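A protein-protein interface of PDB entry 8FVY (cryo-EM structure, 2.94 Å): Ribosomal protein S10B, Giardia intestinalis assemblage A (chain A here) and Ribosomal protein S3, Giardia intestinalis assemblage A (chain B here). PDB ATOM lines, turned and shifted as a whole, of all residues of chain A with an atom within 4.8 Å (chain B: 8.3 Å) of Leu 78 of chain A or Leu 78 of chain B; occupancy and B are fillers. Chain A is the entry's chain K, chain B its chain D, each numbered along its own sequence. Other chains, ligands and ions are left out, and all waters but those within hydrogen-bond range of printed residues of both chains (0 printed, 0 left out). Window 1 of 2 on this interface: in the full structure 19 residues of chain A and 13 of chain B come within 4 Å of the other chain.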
ATOM      1  N   ALA A  20       5.543   2.631  -3.658  1.00  0.00           N
ATOM      2  CA  ALA A  20       5.758   3.423  -4.862  1.00  0.00           C
ATOM      3  C   ALA A  20       5.796   4.917  -4.592  1.00  0.00           C
ATOM      4  O   ALA A  20       5.537   5.715  -5.492  1.00  0.00           O
ATOM      5  CB  ALA A  20       4.686   3.125  -5.899  1.00  0.00           C
ATOM      6  N   SER A  21       6.120   5.329  -3.374  1.00  0.00           N
ATOM      7  CA  SER A  21       6.021   6.737  -3.040  1.00  0.00           C
ATOM      8  C   SER A  21       6.739   7.016  -1.735  1.00  0.00           C
ATOM      9  O   SER A  21       7.299   6.124  -1.097  1.00  0.00           O
ATOM     10  CB  SER A  21       4.568   7.174  -2.943  1.00  0.00           C
ATOM     11  OG  SER A  21       3.840   6.315  -2.098  1.00  0.00           O
ATOM     12  N   LEU A  22       6.716   8.288  -1.358  1.00  0.00           N
ATOM     13  CA  LEU A  22       7.201   8.730  -0.064  1.00  0.00           C
ATOM     14  C   LEU A  22       6.896  10.207   0.100  1.00  0.00           C
ATOM     15  O   LEU A  22       7.454  11.037  -0.616  1.00  0.00           O
ATOM     16  CB  LEU A  22       8.685   8.469   0.068  1.00  0.00           C
ATOM     17  CG  LEU A  22       9.270   8.996   1.365  1.00  0.00           C
ATOM     18  CD1 LEU A  22       8.356   8.678   2.494  1.00  0.00           C
ATOM     19  CD2 LEU A  22      10.618   8.396   1.609  1.00  0.00           C
ATOM     20  N   ALA A  23       6.023  10.528   1.042  1.00  0.00           N
ATOM     21  CA  ALA A  23       5.699  11.903   1.378  1.00  0.00           C
ATOM     22  C   ALA A  23       6.425  12.265   2.658  1.00  0.00           C
ATOM     23  O   ALA A  23       6.173  11.676   3.711  1.00  0.00           O
ATOM     24  CB  ALA A  23       4.199  12.107   1.540  1.00  0.00           C
ATOM     25  N   VAL A  65      15.478   9.213 -10.551  1.00  0.00           N
ATOM     26  CA  VAL A  65      14.654   8.108 -10.093  1.00  0.00           C
ATOM     27  C   VAL A  65      13.253   8.580  -9.754  1.00  0.00           C
ATOM     28  O   VAL A  65      12.263   7.917 -10.076  1.00  0.00           O
ATOM     29  CB  VAL A  65      15.320   7.429  -8.892  1.00  0.00           C
ATOM     30  CG1 VAL A  65      14.397   6.448  -8.299  1.00  0.00           C
ATOM     31  CG2 VAL A  65      16.577   6.770  -9.330  1.00  0.00           C
ATOM     32  N   VAL A  66      13.145   9.717  -9.086  1.00  0.00           N
ATOM     33  CA  VAL A  66      11.861  10.186  -8.597  1.00  0.00           C
ATOM     34  C   VAL A  66      11.578  11.566  -9.150  1.00  0.00           C
ATOM     35  O   VAL A  66      12.427  12.174  -9.807  1.00  0.00           O
ATOM     36  CB  VAL A  66      11.808  10.202  -7.066  1.00  0.00           C
ATOM     37  CG1 VAL A  66      11.670   8.843  -6.564  1.00  0.00           C
ATOM     38  CG2 VAL A  66      13.023  10.807  -6.491  1.00  0.00           C
ATOM     39  N   LYS A  67      10.378  12.066  -8.891  1.00  0.00           N
ATOM     40  CA  LYS A  67       9.978  13.385  -9.345  1.00  0.00           C
ATOM     41  C   LYS A  67       9.203  14.048  -8.220  1.00  0.00           C
ATOM     42  O   LYS A  67       8.158  13.544  -7.801  1.00  0.00           O
ATOM     43  CB  LYS A  67       9.145  13.284 -10.623  1.00  0.00           C
ATOM     44  CG  LYS A  67       7.796  12.666 -10.426  1.00  0.00           C
ATOM     45  CD  LYS A  67       7.340  11.829 -11.623  1.00  0.00           C
ATOM     46  CE  LYS A  67       6.175  10.888 -11.243  1.00  0.00           C
ATOM     47  NZ  LYS A  67       5.845   9.825 -12.224  1.00  0.00           N
ATOM     48  N   THR A  69       7.117  17.033  -6.042  1.00  0.00           N
ATOM     49  CA  THR A  69       5.935  17.850  -6.248  1.00  0.00           C
ATOM     50  C   THR A  69       5.584  18.573  -4.957  1.00  0.00           C
ATOM     51  O   THR A  69       4.497  18.396  -4.406  1.00  0.00           O
ATOM     52  CB  THR A  69       4.777  16.991  -6.729  1.00  0.00           C
ATOM     53  OG1 THR A  69       5.174  16.264  -7.897  1.00  0.00           O
ATOM     54  CG2 THR A  69       3.612  17.849  -7.044  1.00  0.00           C
ATOM     55  N   TYR A  76       6.708  15.428  -1.779  1.00  0.00           N
ATOM     56  CA  TYR A  76       5.964  14.330  -2.367  1.00  0.00           C
ATOM     57  C   TYR A  76       6.756  13.757  -3.522  1.00  0.00           C
ATOM     58  O   TYR A  76       6.842  14.375  -4.585  1.00  0.00           O
ATOM     59  CB  TYR A  76       4.614  14.790  -2.855  1.00  0.00           C
ATOM     60  CG  TYR A  76       3.681  15.241  -1.792  1.00  0.00           C
ATOM     61  CD1 TYR A  76       3.145  14.352  -0.906  1.00  0.00           C
ATOM     62  CD2 TYR A  76       3.293  16.547  -1.712  1.00  0.00           C
ATOM     63  CE1 TYR A  76       2.272  14.763   0.050  1.00  0.00           C
ATOM     64  CE2 TYR A  76       2.431  16.963  -0.768  1.00  0.00           C
ATOM     65  CZ  TYR A  76       1.918  16.075   0.109  1.00  0.00           C
ATOM     66  OH  TYR A  76       1.041  16.530   1.048  1.00  0.00           O
ATOM     67  N   TYR A  77       7.298  12.570  -3.324  1.00  0.00           N
ATOM     68  CA  TYR A  77       8.094  11.883  -4.314  1.00  0.00           C
ATOM     69  C   TYR A  77       7.298  10.741  -4.922  1.00  0.00           C
ATOM     70  O   TYR A  77       6.393  10.190  -4.296  1.00  0.00           O
ATOM     71  CB  TYR A  77       9.366  11.339  -3.706  1.00  0.00           C
ATOM     72  CG  TYR A  77      10.331  12.356  -3.176  1.00  0.00           C
ATOM     73  CD1 TYR A  77      11.058  13.160  -4.026  1.00  0.00           C
ATOM     74  CD2 TYR A  77      10.554  12.481  -1.828  1.00  0.00           C
ATOM     75  CE1 TYR A  77      11.948  14.073  -3.541  1.00  0.00           C
ATOM     76  CE2 TYR A  77      11.445  13.389  -1.343  1.00  0.00           C
ATOM     77  CZ  TYR A  77      12.135  14.180  -2.201  1.00  0.00           C
ATOM     78  OH  TYR A  77      13.024  15.083  -1.706  1.00  0.00           O
ATOM     79  N   LEU A  78       7.629  10.415  -6.165  1.00  0.00           N
ATOM     80  CA  LEU A  78       7.078   9.259  -6.851  1.00  0.00           C
ATOM     81  C   LEU A  78       8.168   8.631  -7.697  1.00  0.00           C
ATOM     82  O   LEU A  78       8.894   9.341  -8.394  1.00  0.00           O
ATOM     83  CB  LEU A  78       5.910   9.636  -7.740  1.00  0.00           C
ATOM     84  CG  LEU A  78       4.740  10.326  -7.088  1.00  0.00           C
ATOM     85  CD1 LEU A  78       4.434  11.571  -7.895  1.00  0.00           C
ATOM     86  CD2 LEU A  78       3.555   9.422  -7.009  1.00  0.00           C
ATOM     87  N   LEU A  79       8.278   7.313  -7.641  1.00  0.00           N
ATOM     88  CA  LEU A  79       9.258   6.615  -8.451  1.00  0.00           C
ATOM     89  C   LEU A  79       8.740   6.462  -9.866  1.00  0.00           C
ATOM     90  O   LEU A  79       7.533   6.342 -10.091  1.00  0.00           O
ATOM     91  CB  LEU A  79       9.599   5.249  -7.863  1.00  0.00           C
ATOM     92  CG  LEU A  79       8.620   4.111  -8.054  1.00  0.00           C
ATOM     93  CD1 LEU A  79       9.144   2.869  -7.426  1.00  0.00           C
ATOM     94  CD2 LEU A  79       7.311   4.473  -7.440  1.00  0.00           C
ATOM     95  N   THR A  80       9.656   6.490 -10.819  1.00  0.00           N
ATOM     96  CA  THR A  80       9.321   6.370 -12.218  1.00  0.00           C
ATOM     97  C   THR A  80       9.647   4.974 -12.734  1.00  0.00           C
ATOM     98  O   THR A  80       9.688   3.992 -11.991  1.00  0.00           O
ATOM     99  CB  THR A  80      10.076   7.413 -13.024  1.00  0.00           C
ATOM    100  OG1 THR A  80      11.410   6.957 -13.259  1.00  0.00           O
ATOM    101  CG2 THR A  80      10.129   8.686 -12.279  1.00  0.00           C
ATOM    102  N   LEU B  27      -4.734  19.090  -0.772  1.00  0.00           N
ATOM    103  CA  LEU B  27      -4.929  18.260  -1.947  1.00  0.00           C
ATOM    104  C   LEU B  27      -5.213  19.104  -3.170  1.00  0.00           C
ATOM    105  O   LEU B  27      -4.747  18.796  -4.268  1.00  0.00           O
ATOM    106  CB  LEU B  27      -6.070  17.300  -1.698  1.00  0.00           C
ATOM    107  CG  LEU B  27      -5.834  16.307  -0.575  1.00  0.00           C
ATOM    108  CD1 LEU B  27      -7.083  15.583  -0.271  1.00  0.00           C
ATOM    109  CD2 LEU B  27      -4.759  15.343  -0.942  1.00  0.00           C
ATOM    110  N   PHE B  30      -1.931  20.325  -4.295  1.00  0.00           N
ATOM    111  CA  PHE B  30      -1.065  19.283  -4.815  1.00  0.00           C
ATOM    112  C   PHE B  30      -1.511  18.842  -6.198  1.00  0.00           C
ATOM    113  O   PHE B  30      -0.701  18.734  -7.125  1.00  0.00           O
ATOM    114  CB  PHE B  30      -1.064  18.122  -3.836  1.00  0.00           C
ATOM    115  CG  PHE B  30      -0.555  16.851  -4.394  1.00  0.00           C
ATOM    116  CD1 PHE B  30       0.783  16.661  -4.617  1.00  0.00           C
ATOM    117  CD2 PHE B  30      -1.416  15.828  -4.653  1.00  0.00           C
ATOM    118  CE1 PHE B  30       1.238  15.481  -5.114  1.00  0.00           C
ATOM    119  CE2 PHE B  30      -0.961  14.656  -5.146  1.00  0.00           C
ATOM    120  CZ  PHE B  30       0.364  14.480  -5.378  1.00  0.00           C
ATOM    121  N   PHE B  31      -2.805  18.601  -6.362  1.00  0.00           N
ATOM    122  CA  PHE B  31      -3.328  18.240  -7.669  1.00  0.00           C
ATOM    123  C   PHE B  31      -3.066  19.340  -8.673  1.00  0.00           C
ATOM    124  O   PHE B  31      -2.639  19.075  -9.801  1.00  0.00           O
ATOM    125  CB  PHE B  31      -4.820  17.984  -7.571  1.00  0.00           C
ATOM    126  CG  PHE B  31      -5.178  16.727  -6.866  1.00  0.00           C
ATOM    127  CD1 PHE B  31      -4.513  15.562  -7.121  1.00  0.00           C
ATOM    128  CD2 PHE B  31      -6.193  16.713  -5.943  1.00  0.00           C
ATOM    129  CE1 PHE B  31      -4.846  14.424  -6.474  1.00  0.00           C
ATOM    130  CE2 PHE B  31      -6.521  15.570  -5.298  1.00  0.00           C
ATOM    131  CZ  PHE B  31      -5.848  14.427  -5.566  1.00  0.00           C
ATOM    132  N   GLU B  34       0.117  19.113  -9.893  1.00  0.00           N
ATOM    133  CA  GLU B  34       0.419  17.795 -10.429  1.00  0.00           C
ATOM    134  C   GLU B  34      -0.369  17.504 -11.700  1.00  0.00           C
ATOM    135  O   GLU B  34       0.198  17.463 -12.794  1.00  0.00           O
ATOM    136  CB  GLU B  34       0.126  16.748  -9.366  1.00  0.00           C
ATOM    137  CG  GLU B  34       0.471  15.349  -9.739  1.00  0.00           C
ATOM    138  CD  GLU B  34       1.770  15.237 -10.491  1.00  0.00           C
ATOM    139  OE1 GLU B  34       1.823  15.682 -11.655  1.00  0.00           O
ATOM    140  OE2 GLU B  34       2.743  14.705  -9.916  1.00  0.00           O
ATOM    141  N   TYR B  70      -2.703   2.790 -12.994  1.00  0.00           N
ATOM    142  CA  TYR B  70      -1.424   2.760 -12.302  1.00  0.00           C
ATOM    143  C   TYR B  70      -1.132   4.084 -11.620  1.00  0.00           C
ATOM    144  O   TYR B  70      -0.730   4.110 -10.456  1.00  0.00           O
ATOM    145  CB  TYR B  70      -0.317   2.415 -13.284  1.00  0.00           C
ATOM    146  CG  TYR B  70       1.005   2.072 -12.655  1.00  0.00           C
ATOM    147  CD1 TYR B  70       1.076   1.513 -11.394  1.00  0.00           C
ATOM    148  CD2 TYR B  70       2.185   2.297 -13.334  1.00  0.00           C
ATOM    149  CE1 TYR B  70       2.290   1.192 -10.822  1.00  0.00           C
ATOM    150  CE2 TYR B  70       3.401   1.978 -12.772  1.00  0.00           C
ATOM    151  CZ  TYR B  70       3.445   1.425 -11.518  1.00  0.00           C
ATOM    152  OH  TYR B  70       4.664   1.118 -10.973  1.00  0.00           O
ATOM    153  N   ARG B  71      -1.324   5.193 -12.325  1.00  0.00           N
ATOM    154  CA  ARG B  71      -1.053   6.494 -11.733  1.00  0.00           C
ATOM    155  C   ARG B  71      -1.950   6.742 -10.531  1.00  0.00           C
ATOM    156  O   ARG B  71      -1.491   7.206  -9.482  1.00  0.00           O
ATOM    157  CB  ARG B  71      -1.245   7.582 -12.782  1.00  0.00           C
ATOM    158  CG  ARG B  71      -0.110   8.581 -12.917  1.00  0.00           C
ATOM    159  CD  ARG B  71      -0.521   9.793 -13.735  1.00  0.00           C
ATOM    160  NE  ARG B  71      -0.131  11.058 -13.123  1.00  0.00           N
ATOM    161  CZ  ARG B  71      -0.215  12.240 -13.723  1.00  0.00           C
ATOM    162  NH1 ARG B  71      -0.560  12.351 -14.991  1.00  0.00           N
ATOM    163  NH2 ARG B  71       0.059  13.342 -13.034  1.00  0.00           N
ATOM    164  N   LEU B  72      -3.231   6.418 -10.661  1.00  0.00           N
ATOM    165  CA  LEU B  72      -4.167   6.588  -9.560  1.00  0.00           C
ATOM    166  C   LEU B  72      -3.714   5.814  -8.336  1.00  0.00           C
ATOM    167  O   LEU B  72      -3.728   6.327  -7.212  1.00  0.00           O
ATOM    168  CB  LEU B  72      -5.538   6.098  -9.986  1.00  0.00           C
ATOM    169  CG  LEU B  72      -6.764   6.916  -9.613  1.00  0.00           C
ATOM    170  CD1 LEU B  72      -6.771   8.183 -10.385  1.00  0.00           C
ATOM    171  CD2 LEU B  72      -8.013   6.138  -9.865  1.00  0.00           C
ATOM    172  N   HIS B  73      -3.333   4.559  -8.537  1.00  0.00           N
ATOM    173  CA  HIS B  73      -2.946   3.713  -7.423  1.00  0.00           C
ATOM    174  C   HIS B  73      -1.645   4.181  -6.810  1.00  0.00           C
ATOM    175  O   HIS B  73      -1.478   4.161  -5.587  1.00  0.00           O
ATOM    176  CB  HIS B  73      -2.851   2.280  -7.905  1.00  0.00           C
ATOM    177  CG  HIS B  73      -4.175   1.676  -8.234  1.00  0.00           C
ATOM    178  ND1 HIS B  73      -4.390   0.923  -9.365  1.00  0.00           N
ATOM    179  CD2 HIS B  73      -5.357   1.717  -7.579  1.00  0.00           C
ATOM    180  CE1 HIS B  73      -5.648   0.523  -9.392  1.00  0.00           C
ATOM    181  NE2 HIS B  73      -6.258   0.992  -8.320  1.00  0.00           N
ATOM    182  N   LYS B  74      -0.715   4.619  -7.646  1.00  0.00           N
ATOM    183  CA  LYS B  74       0.521   5.195  -7.145  1.00  0.00           C
ATOM    184  C   LYS B  74       0.219   6.393  -6.270  1.00  0.00           C
ATOM    185  O   LYS B  74       0.928   6.672  -5.299  1.00  0.00           O
ATOM    186  CB  LYS B  74       1.406   5.605  -8.307  1.00  0.00           C
ATOM    187  CG  LYS B  74       2.802   5.162  -8.167  1.00  0.00           C
ATOM    188  CD  LYS B  74       3.718   5.789  -9.210  1.00  0.00           C
ATOM    189  CE  LYS B  74       3.152   5.719 -10.572  1.00  0.00           C
ATOM    190  NZ  LYS B  74       2.792   4.333 -10.850  1.00  0.00           N
ATOM    191  N   ILE B  75      -0.828   7.126  -6.624  1.00  0.00           N
ATOM    192  CA  ILE B  75      -1.218   8.296  -5.853  1.00  0.00           C
ATOM    193  C   ILE B  75      -1.808   7.882  -4.516  1.00  0.00           C
ATOM    194  O   ILE B  75      -1.514   8.475  -3.475  1.00  0.00           O
ATOM    195  CB  ILE B  75      -2.210   9.144  -6.650  1.00  0.00           C
ATOM    196  CG1 ILE B  75      -1.509   9.910  -7.758  1.00  0.00           C
ATOM    197  CG2 ILE B  75      -2.856  10.069  -5.745  1.00  0.00           C
ATOM    198  CD1 ILE B  75      -0.614  10.978  -7.297  1.00  0.00           C
ATOM    199  N   GLU B  76      -2.674   6.876  -4.527  1.00  0.00           N
ATOM    200  CA  GLU B  76      -3.400   6.522  -3.315  1.00  0.00           C
ATOM    201  C   GLU B  76      -2.448   6.136  -2.200  1.00  0.00           C
ATOM    202  O   GLU B  76      -2.579   6.597  -1.064  1.00  0.00           O
ATOM    203  CB  GLU B  76      -4.353   5.377  -3.597  1.00  0.00           C
ATOM    204  CG  GLU B  76      -5.542   5.747  -4.421  1.00  0.00           C
ATOM    205  CD  GLU B  76      -6.383   4.551  -4.799  1.00  0.00           C
ATOM    206  OE1 GLU B  76      -6.015   3.422  -4.417  1.00  0.00           O
ATOM    207  OE2 GLU B  76      -7.410   4.737  -5.484  1.00  0.00           O
ATOM    208  N   TYR B  77      -1.486   5.272  -2.503  1.00  0.00           N
ATOM    209  CA  TYR B  77      -0.529   4.853  -1.491  1.00  0.00           C
ATOM    210  C   TYR B  77       0.261   6.032  -0.959  1.00  0.00           C
ATOM    211  O   TYR B  77       0.703   6.029   0.192  1.00  0.00           O
ATOM    212  CB  TYR B  77       0.404   3.805  -2.080  1.00  0.00           C
ATOM    213  CG  TYR B  77      -0.131   2.405  -1.961  1.00  0.00           C
ATOM    214  CD1 TYR B  77      -1.244   2.007  -2.675  1.00  0.00           C
ATOM    215  CD2 TYR B  77       0.471   1.488  -1.130  1.00  0.00           C
ATOM    216  CE1 TYR B  77      -1.731   0.743  -2.567  1.00  0.00           C
ATOM    217  CE2 TYR B  77      -0.012   0.222  -1.017  1.00  0.00           C
ATOM    218  CZ  TYR B  77      -1.114  -0.148  -1.737  1.00  0.00           C
ATOM    219  OH  TYR B  77      -1.600  -1.423  -1.621  1.00  0.00           O
ATOM    220  N   LEU B  78       0.446   7.049  -1.790  1.00  0.00           N
ATOM    221  CA  LEU B  78       1.253   8.196  -1.414  1.00  0.00           C
ATOM    222  C   LEU B  78       0.546   9.054  -0.385  1.00  0.00           C
ATOM    223  O   LEU B  78       1.097   9.373   0.672  1.00  0.00           O
ATOM    224  CB  LEU B  78       1.552   9.008  -2.655  1.00  0.00           C
ATOM    225  CG  LEU B  78       1.935  10.455  -2.471  1.00  0.00           C
ATOM    226  CD1 LEU B  78       3.134  10.564  -1.633  1.00  0.00           C
ATOM    227  CD2 LEU B  78       2.183  11.058  -3.802  1.00  0.00           C
ATOM    228  N   LEU B  79      -0.679   9.448  -0.691  1.00  0.00           N
ATOM    229  CA  LEU B  79      -1.420  10.325   0.195  1.00  0.00           C
ATOM    230  C   LEU B  79      -1.555   9.704   1.569  1.00  0.00           C
ATOM    231  O   LEU B  79      -1.486  10.397   2.589  1.00  0.00           O
ATOM    232  CB  LEU B  79      -2.787  10.592  -0.412  1.00  0.00           C
ATOM    233  CG  LEU B  79      -2.793  11.402  -1.706  1.00  0.00           C
ATOM    234  CD1 LEU B  79      -4.163  11.864  -2.091  1.00  0.00           C
ATOM    235  CD2 LEU B  79      -1.897  12.575  -1.582  1.00  0.00           C
ATOM    236  N   ALA B  80      -1.717   8.388   1.613  1.00  0.00           N
ATOM    237  CA  ALA B  80      -2.013   7.710   2.859  1.00  0.00           C
ATOM    238  C   ALA B  80      -0.865   7.849   3.835  1.00  0.00           C
ATOM    239  O   ALA B  80      -1.064   8.095   5.029  1.00  0.00           O
ATOM    240  CB  ALA B  80      -2.295   6.256   2.572  1.00  0.00           C
ATOM    241  N   GLY B  81       0.352   7.689   3.337  1.00  0.00           N
ATOM    242  CA  GLY B  81       1.507   7.902   4.182  1.00  0.00           C
ATOM    243  C   GLY B  81       1.528   9.293   4.772  1.00  0.00           C
ATOM    244  O   GLY B  81       1.834   9.475   5.952  1.00  0.00           O
ATOM    245  N   ARG B  82       1.188  10.292   3.966  1.00  0.00           N
ATOM    246  CA  ARG B  82       1.241  11.662   4.445  1.00  0.00           C
ATOM    247  C   ARG B  82       0.155  11.927   5.469  1.00  0.00           C
ATOM    248  O   ARG B  82       0.413  12.526   6.516  1.00  0.00           O
ATOM    249  CB  ARG B  82       1.120  12.614   3.271  1.00  0.00           C
ATOM    250  CG  ARG B  82       1.350  14.059   3.634  1.00  0.00           C
ATOM    251  CD  ARG B  82       0.081  14.787   3.820  1.00  0.00           C
ATOM    252  NE  ARG B  82       0.241  15.994   4.609  1.00  0.00           N
ATOM    253  CZ  ARG B  82       0.265  16.013   5.931  1.00  0.00           C
ATOM    254  NH1 ARG B  82       0.349  14.902   6.634  1.00  0.00           N
ATOM    255  NH2 ARG B  82       0.202  17.175   6.561  1.00  0.00           N
ATOM    256  N   PHE B  83      -1.064  11.497   5.188  1.00  0.00           N
ATOM    257  CA  PHE B  83      -2.160  11.664   6.122  1.00  0.00           C
ATOM    258  C   PHE B  83      -2.284  10.486   7.058  1.00  0.00           C
ATOM    259  O   PHE B  83      -3.186  10.462   7.899  1.00  0.00           O
ATOM    260  CB  PHE B  83      -3.460  11.878   5.367  1.00  0.00           C
ATOM    261  CG  PHE B  83      -3.461  13.112   4.532  1.00  0.00           C
ATOM    262  CD1 PHE B  83      -3.132  14.330   5.086  1.00  0.00           C
ATOM    263  CD2 PHE B  83      -3.762  13.060   3.190  1.00  0.00           C
ATOM    264  CE1 PHE B  83      -3.109  15.463   4.322  1.00  0.00           C
ATOM    265  CE2 PHE B  83      -3.741  14.196   2.426  1.00  0.00           C
ATOM    266  CZ  PHE B  83      -3.415  15.397   2.993  1.00  0.00           C
ATOM    267  N   MET B  84      -1.391   9.512   6.932  1.00  0.00           N
ATOM    268  CA  MET B  84      -1.288   8.424   7.889  1.00  0.00           C
ATOM    269  C   MET B  84      -2.617   7.687   8.016  1.00  0.00           C
ATOM    270  O   MET B  84      -3.244   7.648   9.075  1.00  0.00           O
ATOM    271  CB  MET B  84      -0.802   8.937   9.238  1.00  0.00           C
ATOM    272  CG  MET B  84       0.685   9.062   9.296  1.00  0.00           C
ATOM    273  SD  MET B  84       1.332  10.665   8.820  1.00  0.00           S
ATOM    274  CE  MET B  84       0.879  11.626  10.244  1.00  0.00           C
ATOM    275  N   CYS B  85      -3.044   7.110   6.907  1.00  0.00           N
ATOM    276  CA  CYS B  85      -4.167   6.199   6.871  1.00  0.00           C
ATOM    277  C   CYS B  85      -3.676   4.882   6.302  1.00  0.00           C
ATOM    278  O   CYS B  85      -2.680   4.844   5.578  1.00  0.00           O
ATOM    279  CB  CYS B  85      -5.312   6.745   6.025  1.00  0.00           C
ATOM    280  SG  CYS B  85      -6.657   5.570   5.796  1.00  0.00           S
ATOM    281  N   PRO B  87      -3.350   2.317   3.739  1.00  0.00           N
ATOM    282  CA  PRO B  87      -3.686   2.256   2.318  1.00  0.00           C
ATOM    283  C   PRO B  87      -4.653   1.120   2.056  1.00  0.00           C
ATOM    284  O   PRO B  87      -4.777   0.175   2.834  1.00  0.00           O
ATOM    285  CB  PRO B  87      -2.344   2.033   1.628  1.00  0.00           C
ATOM    286  CG  PRO B  87      -1.437   1.552   2.685  1.00  0.00           C
ATOM    287  CD  PRO B  87      -1.905   2.170   3.954  1.00  0.00           C
ATOM    288  N   PHE B  90      -7.826   4.277   1.303  1.00  0.00           N
ATOM    289  CA  PHE B  90      -7.655   5.602   0.729  1.00  0.00           C
ATOM    290  C   PHE B  90      -7.973   5.580  -0.756  1.00  0.00           C
ATOM    291  O   PHE B  90      -7.153   5.960  -1.591  1.00  0.00           O
ATOM    292  CB  PHE B  90      -6.236   6.106   0.955  1.00  0.00           C
ATOM    293  CG  PHE B  90      -6.119   7.592   0.974  1.00  0.00           C
ATOM    294  CD1 PHE B  90      -6.026   8.290  -0.203  1.00  0.00           C
ATOM    295  CD2 PHE B  90      -6.068   8.289   2.167  1.00  0.00           C
ATOM    296  CE1 PHE B  90      -5.912   9.646  -0.201  1.00  0.00           C
ATOM    297  CE2 PHE B  90      -5.950   9.654   2.171  1.00  0.00           C
ATOM    298  CZ  PHE B  90      -5.869  10.332   0.985  1.00  0.00           C
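The backbone NH (N) of Lys 67 of chain A lies within hydrogen-bond range of the backbone carbonyl oxygen (O) of Leu 78 of chain A, 3.1 Å away. O of Tyr 76 of chain A is in hydrogen-bond range of N of Thr 69 of chain A. OE1 of Glu 34 of chain B is in salt-bridge range of NH2 of Arg 71 of chain B.
OG of Ser 21 of chain A lies close to N of Leu 78 of chain B, at 3.5 Å.
Hydrophobic or aromatic side chains of chain B that line the printed part of chain A: Phe 30 and Leu 78. Of the 13 printed residues of chain A, 7 touch a printed residue of chain B. Along chain A the printed residues that touch a printed residue of chain B span positions 20 to 79. Among the printed residues, no Asp or Glu carboxylate lies within 4 Å of a Lys or Arg side-chain nitrogen of the other chain.
Of the printed residues of chain B, Ala 23 of chain A touches Leu 78 and Arg 82. Of the printed residues of chain B, Tyr 76 of chain A touches Phe 30, Leu 78 and Arg 82. Leu 78 of chain A touches just one residue of chain B: Leu 78. Of the printed residues of chain A, Glu 34 of chain B touches Thr 69 (3.5 Å). Glu 76 of chain B touches none of the printed residues of chain A. Leu 78 of chain B touches just these residues of chain A: Ser 21 (3.3 Å), Ala 23 (3.7 Å), Tyr 76 (3.9 Å) and Leu 78 (3.9 Å). The nearest residue of chain A that does not touch Leu 78 of chain B is Leu 22 of chain A (4.2 Å). The nearest printed residue of chain B that does not touch Ala 20 of chain A is Tyr 70 of chain B (5.5 Å).
CB of Ala 20 of chain A touches CG of Lys 74 of chain B, 3.6 Å away. Ser 21 of chain A touches Tyr 77 of chain B (OG to C, 3.8 Å). Ala 23 of chain A touches Leu 78 of chain B. Arg 82 of chain B touches Ala 23 of chain A (CB to CB, 3.6 Å). Phe 30 of chain B touches Thr 69 of chain A. CD1 of Phe 30 of chain B touches CD2 of Tyr 76 of chain A, at 3.8 Å. Tyr 76 of chain A touches Leu 78 of chain B (CD1 to CD1, 3.9 Å). Tyr 76 of chain A touches Arg 82 of chain B (OH to CD, 3.4 Å). Leu 78 of chain A touches Leu 78 of chain B (CD2 to CD2, 3.9 Å). O of Leu 79 of chain A touches CD of Lys 74 of chain B (3.95 Å).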
